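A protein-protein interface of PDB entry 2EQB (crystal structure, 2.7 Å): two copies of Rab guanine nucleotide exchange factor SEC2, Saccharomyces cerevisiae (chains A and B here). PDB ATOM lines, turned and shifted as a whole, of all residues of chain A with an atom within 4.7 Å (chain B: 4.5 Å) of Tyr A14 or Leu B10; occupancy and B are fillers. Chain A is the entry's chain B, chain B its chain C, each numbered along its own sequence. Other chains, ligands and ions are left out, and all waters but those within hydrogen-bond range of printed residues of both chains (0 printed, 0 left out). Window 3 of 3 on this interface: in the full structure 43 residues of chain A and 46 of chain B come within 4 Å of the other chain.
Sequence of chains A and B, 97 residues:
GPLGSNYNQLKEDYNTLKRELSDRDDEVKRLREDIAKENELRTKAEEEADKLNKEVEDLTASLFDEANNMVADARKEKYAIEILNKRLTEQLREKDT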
ATOM      1  N   TYR A   7     -22.101   0.158   1.767  1.00  0.00           N
ATOM      2  CA  TYR A   7     -22.215  -0.254   3.172  1.00  0.00           C
ATOM      3  C   TYR A   7     -23.289   0.486   3.956  1.00  0.00           C
ATOM      4  O   TYR A   7     -23.918  -0.076   4.856  1.00  0.00           O
ATOM      5  CB  TYR A   7     -20.898  -0.105   3.915  1.00  0.00           C
ATOM      6  CG  TYR A   7     -21.022  -0.535   5.367  1.00  0.00           C
ATOM      7  CD1 TYR A   7     -20.677  -1.825   5.769  1.00  0.00           C
ATOM      8  CD2 TYR A   7     -21.540   0.334   6.328  1.00  0.00           C
ATOM      9  CE1 TYR A   7     -20.844  -2.238   7.098  1.00  0.00           C
ATOM     10  CE2 TYR A   7     -21.716  -0.069   7.646  1.00  0.00           C
ATOM     11  CZ  TYR A   7     -21.365  -1.351   8.027  1.00  0.00           C
ATOM     12  OH  TYR A   7     -21.533  -1.742   9.338  1.00  0.00           O
ATOM     13  N   LEU A  10     -26.781  -0.766   2.880  1.00  0.00           N
ATOM     14  CA  LEU A  10     -26.941  -2.125   3.381  1.00  0.00           C
ATOM     15  C   LEU A  10     -27.371  -2.114   4.843  1.00  0.00           C
ATOM     16  O   LEU A  10     -28.447  -2.608   5.175  1.00  0.00           O
ATOM     17  CB  LEU A  10     -25.642  -2.924   3.255  1.00  0.00           C
ATOM     18  CG  LEU A  10     -25.724  -4.332   3.849  1.00  0.00           C
ATOM     19  CD1 LEU A  10     -26.708  -5.124   3.034  1.00  0.00           C
ATOM     20  CD2 LEU A  10     -24.383  -5.022   3.837  1.00  0.00           C
ATOM     21  N   LYS A  11     -26.543  -1.552   5.719  1.00  0.00           N
ATOM     22  CA  LYS A  11     -26.900  -1.515   7.135  1.00  0.00           C
ATOM     23  C   LYS A  11     -28.280  -0.874   7.330  1.00  0.00           C
ATOM     24  O   LYS A  11     -29.013  -1.238   8.254  1.00  0.00           O
ATOM     25  CB  LYS A  11     -25.854  -0.750   7.963  1.00  0.00           C
ATOM     26  CG  LYS A  11     -25.934  -1.055   9.479  1.00  0.00           C
ATOM     27  CD  LYS A  11     -25.260   0.013  10.354  1.00  0.00           C
ATOM     28  CE  LYS A  11     -26.012   1.350  10.271  1.00  0.00           C
ATOM     29  NZ  LYS A  11     -25.370   2.478  11.017  1.00  0.00           N
ATOM     30  N   GLU A  12     -28.640   0.079   6.470  1.00  0.00           N
ATOM     31  CA  GLU A  12     -29.945   0.738   6.591  1.00  0.00           C
ATOM     32  C   GLU A  12     -30.998  -0.294   6.241  1.00  0.00           C
ATOM     33  O   GLU A  12     -31.973  -0.488   6.972  1.00  0.00           O
ATOM     34  CB  GLU A  12     -30.052   1.929   5.633  1.00  0.00           C
ATOM     35  CG  GLU A  12     -31.275   2.814   5.864  1.00  0.00           C
ATOM     36  CD  GLU A  12     -31.194   4.127   5.100  1.00  0.00           C
ATOM     37  OE1 GLU A  12     -30.291   4.933   5.408  1.00  0.00           O
ATOM     38  OE2 GLU A  12     -32.028   4.352   4.193  1.00  0.00           O
ATOM     39  N   ASP A  13     -30.767  -0.963   5.115  1.00  0.00           N
ATOM     40  CA  ASP A  13     -31.661  -1.997   4.621  1.00  0.00           C
ATOM     41  C   ASP A  13     -31.818  -3.116   5.619  1.00  0.00           C
ATOM     42  O   ASP A  13     -32.930  -3.567   5.886  1.00  0.00           O
ATOM     43  CB  ASP A  13     -31.143  -2.554   3.305  1.00  0.00           C
ATOM     44  CG  ASP A  13     -31.369  -1.608   2.151  1.00  0.00           C
ATOM     45  OD1 ASP A  13     -32.173  -0.663   2.309  1.00  0.00           O
ATOM     46  OD2 ASP A  13     -30.755  -1.817   1.085  1.00  0.00           O
ATOM     47  N   TYR A  14     -30.695  -3.565   6.161  1.00  0.00           N
ATOM     48  CA  TYR A  14     -30.717  -4.617   7.158  1.00  0.00           C
ATOM     49  C   TYR A  14     -31.577  -4.167   8.340  1.00  0.00           C
ATOM     50  O   TYR A  14     -32.350  -4.957   8.893  1.00  0.00           O
ATOM     51  CB  TYR A  14     -29.307  -4.902   7.655  1.00  0.00           C
ATOM     52  CG  TYR A  14     -29.239  -5.937   8.754  1.00  0.00           C
ATOM     53  CD1 TYR A  14     -29.565  -7.272   8.503  1.00  0.00           C
ATOM     54  CD2 TYR A  14     -28.777  -5.599  10.025  1.00  0.00           C
ATOM     55  CE1 TYR A  14     -29.419  -8.245   9.486  1.00  0.00           C
ATOM     56  CE2 TYR A  14     -28.628  -6.568  11.023  1.00  0.00           C
ATOM     57  CZ  TYR A  14     -28.941  -7.888  10.745  1.00  0.00           C
ATOM     58  OH  TYR A  14     -28.726  -8.859  11.697  1.00  0.00           O
ATOM     59  N   ASN A  15     -31.432  -2.905   8.746  1.00  0.00           N
ATOM     60  CA  ASN A  15     -32.218  -2.394   9.869  1.00  0.00           C
ATOM     61  C   ASN A  15     -33.689  -2.371   9.485  1.00  0.00           C
ATOM     62  O   ASN A  15     -34.566  -2.604  10.317  1.00  0.00           O
ATOM     63  CB  ASN A  15     -31.757  -0.988  10.272  1.00  0.00           C
ATOM     64  CG  ASN A  15     -30.532  -1.014  11.159  1.00  0.00           C
ATOM     65  OD1 ASN A  15     -30.108  -2.080  11.600  1.00  0.00           O
ATOM     66  ND2 ASN A  15     -29.960   0.158  11.438  1.00  0.00           N
ATOM     67  N   THR A  16     -33.951  -2.100   8.211  1.00  0.00           N
ATOM     68  CA  THR A  16     -35.313  -2.059   7.710  1.00  0.00           C
ATOM     69  C   THR A  16     -35.901  -3.467   7.693  1.00  0.00           C
ATOM     70  O   THR A  16     -37.007  -3.705   8.185  1.00  0.00           O
ATOM     71  CB  THR A  16     -35.348  -1.445   6.302  1.00  0.00           C
ATOM     72  OG1 THR A  16     -35.444  -0.020   6.410  1.00  0.00           O
ATOM     73  CG2 THR A  16     -36.520  -1.972   5.514  1.00  0.00           C
ATOM     74  N   LEU A  17     -35.170  -4.407   7.112  1.00  0.00           N
ATOM     75  CA  LEU A  17     -35.641  -5.781   7.099  1.00  0.00           C
ATOM     76  C   LEU A  17     -35.875  -6.165   8.559  1.00  0.00           C
ATOM     77  O   LEU A  17     -36.945  -6.633   8.924  1.00  0.00           O
ATOM     78  CB  LEU A  17     -34.587  -6.697   6.496  1.00  0.00           C
ATOM     79  CG  LEU A  17     -34.896  -8.176   6.708  1.00  0.00           C
ATOM     80  CD1 LEU A  17     -35.318  -8.759   5.382  1.00  0.00           C
ATOM     81  CD2 LEU A  17     -33.681  -8.914   7.266  1.00  0.00           C
ATOM     82  N   LYS A  18     -34.859  -5.953   9.389  1.00  0.00           N
ATOM     83  CA  LYS A  18     -34.949  -6.257  10.810  1.00  0.00           C
ATOM     84  C   LYS A  18     -36.319  -5.913  11.399  1.00  0.00           C
ATOM     85  O   LYS A  18     -36.876  -6.683  12.185  1.00  0.00           O
ATOM     86  CB  LYS A  18     -33.872  -5.489  11.579  1.00  0.00           C
ATOM     87  CG  LYS A  18     -32.734  -6.352  12.084  1.00  0.00           C
ATOM     88  CD  LYS A  18     -31.924  -5.659  13.180  1.00  0.00           C
ATOM     89  CE  LYS A  18     -31.180  -4.444  12.654  1.00  0.00           C
ATOM     90  NZ  LYS A  18     -30.500  -3.702  13.760  1.00  0.00           N
ATOM     91  N   ASN B   6     -16.619  -8.394   9.136  1.00  0.00           N
ATOM     92  CA  ASN B   6     -17.765  -7.746   9.741  1.00  0.00           C
ATOM     93  C   ASN B   6     -18.695  -7.457   8.557  1.00  0.00           C
ATOM     94  O   ASN B   6     -19.880  -7.760   8.608  1.00  0.00           O
ATOM     95  CB  ASN B   6     -17.348  -6.461  10.448  1.00  0.00           C
ATOM     96  CG  ASN B   6     -17.136  -6.666  11.923  1.00  0.00           C
ATOM     97  OD1 ASN B   6     -16.655  -7.718  12.351  1.00  0.00           O
ATOM     98  ND2 ASN B   6     -17.490  -5.661  12.716  1.00  0.00           N
ATOM     99  N   TYR B   7     -18.152  -6.910   7.471  1.00  0.00           N
ATOM    100  CA  TYR B   7     -18.987  -6.647   6.307  1.00  0.00           C
ATOM    101  C   TYR B   7     -19.650  -7.942   5.809  1.00  0.00           C
ATOM    102  O   TYR B   7     -20.869  -8.016   5.680  1.00  0.00           O
ATOM    103  CB  TYR B   7     -18.168  -6.046   5.163  1.00  0.00           C
ATOM    104  CG  TYR B   7     -18.976  -5.770   3.887  1.00  0.00           C
ATOM    105  CD1 TYR B   7     -19.592  -4.535   3.669  1.00  0.00           C
ATOM    106  CD2 TYR B   7     -19.066  -6.723   2.876  1.00  0.00           C
ATOM    107  CE1 TYR B   7     -20.264  -4.261   2.474  1.00  0.00           C
ATOM    108  CE2 TYR B   7     -19.730  -6.457   1.685  1.00  0.00           C
ATOM    109  CZ  TYR B   7     -20.323  -5.227   1.485  1.00  0.00           C
ATOM    110  OH  TYR B   7     -20.949  -4.960   0.288  1.00  0.00           O
ATOM    111  N   ASN B   8     -18.846  -8.958   5.525  1.00  0.00           N
ATOM    112  CA  ASN B   8     -19.404 -10.205   5.030  1.00  0.00           C
ATOM    113  C   ASN B   8     -20.425 -10.829   5.976  1.00  0.00           C
ATOM    114  O   ASN B   8     -21.433 -11.381   5.524  1.00  0.00           O
ATOM    115  CB  ASN B   8     -18.287 -11.206   4.713  1.00  0.00           C
ATOM    116  CG  ASN B   8     -17.505 -10.825   3.463  1.00  0.00           C
ATOM    117  OD1 ASN B   8     -18.021 -10.143   2.567  1.00  0.00           O
ATOM    118  ND2 ASN B   8     -16.260 -11.279   3.389  1.00  0.00           N
ATOM    119  N   GLN B   9     -20.183 -10.737   7.279  1.00  0.00           N
ATOM    120  CA  GLN B   9     -21.117 -11.308   8.250  1.00  0.00           C
ATOM    121  C   GLN B   9     -22.472 -10.630   8.111  1.00  0.00           C
ATOM    122  O   GLN B   9     -23.515 -11.281   8.090  1.00  0.00           O
ATOM    123  CB  GLN B   9     -20.606 -11.111   9.671  1.00  0.00           C
ATOM    124  CG  GLN B   9     -21.492 -11.758  10.712  1.00  0.00           C
ATOM    125  CD  GLN B   9     -21.742 -13.220  10.408  1.00  0.00           C
ATOM    126  OE1 GLN B   9     -20.835 -13.937   9.983  1.00  0.00           O
ATOM    127  NE2 GLN B   9     -22.971 -13.673  10.633  1.00  0.00           N
ATOM    128  N   LEU B  10     -22.441  -9.305   8.039  1.00  0.00           N
ATOM    129  CA  LEU B  10     -23.649  -8.521   7.875  1.00  0.00           C
ATOM    130  C   LEU B  10     -24.340  -9.024   6.624  1.00  0.00           C
ATOM    131  O   LEU B  10     -25.467  -9.506   6.666  1.00  0.00           O
ATOM    132  CB  LEU B  10     -23.316  -7.047   7.663  1.00  0.00           C
ATOM    133  CG  LEU B  10     -24.553  -6.198   7.371  1.00  0.00           C
ATOM    134  CD1 LEU B  10     -25.332  -6.045   8.668  1.00  0.00           C
ATOM    135  CD2 LEU B  10     -24.175  -4.844   6.839  1.00  0.00           C
ATOM    136  N   LYS B  11     -23.636  -8.913   5.506  1.00  0.00           N
ATOM    137  CA  LYS B  11     -24.187  -9.324   4.230  1.00  0.00           C
ATOM    138  C   LYS B  11     -24.944 -10.632   4.341  1.00  0.00           C
ATOM    139  O   LYS B  11     -25.908 -10.851   3.599  1.00  0.00           O
ATOM    140  CB  LYS B  11     -23.081  -9.437   3.168  1.00  0.00           C
ATOM    141  CG  LYS B  11     -23.502  -8.831   1.835  1.00  0.00           C
ATOM    142  CD  LYS B  11     -22.342  -8.645   0.879  1.00  0.00           C
ATOM    143  CE  LYS B  11     -22.797  -7.830  -0.331  1.00  0.00           C
ATOM    144  NZ  LYS B  11     -21.687  -7.518  -1.274  1.00  0.00           N
ATOM    145  N   GLU B  12     -24.541 -11.481   5.288  1.00  0.00           N
ATOM    146  CA  GLU B  12     -25.198 -12.779   5.444  1.00  0.00           C
ATOM    147  C   GLU B  12     -26.302 -12.853   6.503  1.00  0.00           C
ATOM    148  O   GLU B  12     -27.227 -13.671   6.386  1.00  0.00           O
ATOM    149  CB  GLU B  12     -24.156 -13.869   5.703  1.00  0.00           C
ATOM    150  CG  GLU B  12     -23.912 -14.199   7.161  1.00  0.00           C
ATOM    151  CD  GLU B  12     -23.283 -15.561   7.296  1.00  0.00           C
ATOM    152  OE1 GLU B  12     -23.043 -16.027   8.435  1.00  0.00           O
ATOM    153  OE2 GLU B  12     -23.037 -16.161   6.229  1.00  0.00           O
ATOM    154  N   ASP B  13     -26.196 -12.034   7.548  1.00  0.00           N
ATOM    155  CA  ASP B  13     -27.231 -12.020   8.566  1.00  0.00           C
ATOM    156  C   ASP B  13     -28.414 -11.427   7.841  1.00  0.00           C
ATOM    157  O   ASP B  13     -29.569 -11.787   8.089  1.00  0.00           O
ATOM    158  CB  ASP B  13     -26.830 -11.154   9.762  1.00  0.00           C
ATOM    159  CG  ASP B  13     -25.825 -11.850  10.661  1.00  0.00           C
ATOM    160  OD1 ASP B  13     -25.562 -13.037  10.405  1.00  0.00           O
ATOM    161  OD2 ASP B  13     -25.303 -11.237  11.618  1.00  0.00           O
ATOM    162  N   TYR B  14     -28.118 -10.526   6.915  1.00  0.00           N
ATOM    163  CA  TYR B  14     -29.183  -9.933   6.147  1.00  0.00           C
ATOM    164  C   TYR B  14     -29.843 -11.066   5.400  1.00  0.00           C
ATOM    165  O   TYR B  14     -31.069 -11.120   5.300  1.00  0.00           O
ATOM    166  CB  TYR B  14     -28.676  -8.930   5.138  1.00  0.00           C
ATOM    167  CG  TYR B  14     -29.797  -8.382   4.275  1.00  0.00           C
ATOM    168  CD1 TYR B  14     -30.392  -7.153   4.564  1.00  0.00           C
ATOM    169  CD2 TYR B  14     -30.238  -9.077   3.149  1.00  0.00           C
ATOM    170  CE1 TYR B  14     -31.394  -6.621   3.739  1.00  0.00           C
ATOM    171  CE2 TYR B  14     -31.233  -8.556   2.321  1.00  0.00           C
ATOM    172  CZ  TYR B  14     -31.802  -7.327   2.619  1.00  0.00           C
ATOM    173  OH  TYR B  14     -32.745  -6.789   1.781  1.00  0.00           O
ATOM    174  N   LEU B  17     -31.925 -13.484   7.935  1.00  0.00           N
ATOM    175  CA  LEU B  17     -33.243 -12.998   8.312  1.00  0.00           C
ATOM    176  C   LEU B  17     -34.098 -12.734   7.073  1.00  0.00           C
ATOM    177  O   LEU B  17     -35.311 -12.704   7.156  1.00  0.00           O
ATOM    178  CB  LEU B  17     -33.138 -11.717   9.135  1.00  0.00           C
ATOM    179  CG  LEU B  17     -32.185 -11.638  10.330  1.00  0.00           C
ATOM    180  CD1 LEU B  17     -32.489 -10.319  10.946  1.00  0.00           C
ATOM    181  CD2 LEU B  17     -32.356 -12.733  11.384  1.00  0.00           C
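The side-chain hydroxyl of Tyr B7 lies within hydrogen-bond range of the side-chain amino group of Lys B11 (3.1 Å). The side-chain amide nitrogen (NE2) of Gln B9 lies within hydrogen-bond range of the side-chain carboxylate (OD1) of Asp B13 (2.7 Å).
Among the printed residues, merely in contact across the chains: Tyr A7 with Tyr B7, Leu A10 with Leu B10, Asp A13 with Tyr B14, Tyr A14 with Leu B10, Tyr A14 with Asp B13, Tyr A14 with Tyr B14, Tyr A14 with Leu B17, Leu A17 with Tyr B14 and Leu A17 with Leu B17.
Of the printed residues of chain B, Tyr A14 touches Leu B10, Asp B13, Tyr B14 and Leu B17. Printed residues of chain A within 4 Å of Leu B10: Leu A10 (3.0 Å) and Tyr A14 (3.7 Å). Printed residues of chain A within 4 Å of Asp B13: Tyr A14 (3.6 Å). Of the printed residues of chain A, Tyr B14 touches Asp A13, Tyr A14 and Leu A17. The nearest residue of chain A that does not touch Leu B10 is Lys A11 (4.2 Å). The nearest printed residue of chain B that does not touch Tyr A7 is Leu B10 (4.2 Å).
Hydrophobic or aromatic side chains of chain B that line the printed part of chain A: Tyr B7, Leu B10, Tyr B14 and Leu B17. Of the 10 printed residues of chain A, 5 touch a printed residue of chain B. Among the printed residues, no Asp or Glu carboxylate lies within 4 Å of a Lys or Arg side-chain nitrogen of the other chain.
Leu B10 touches its own counterpart, Leu A10. Asp A13 touches Tyr B14, and with the chains exchanged Tyr A14 touches Asp B13. Tyr A14 touches Leu B10, but with the chains exchanged Leu A10 does not touch Tyr B14 (4.5 Å). Leu A17 touches its own counterpart, Leu B17. Of the 9 pairs that touch across the chains among the printed residues, 8 have their exchanged pair printed and touching as well.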
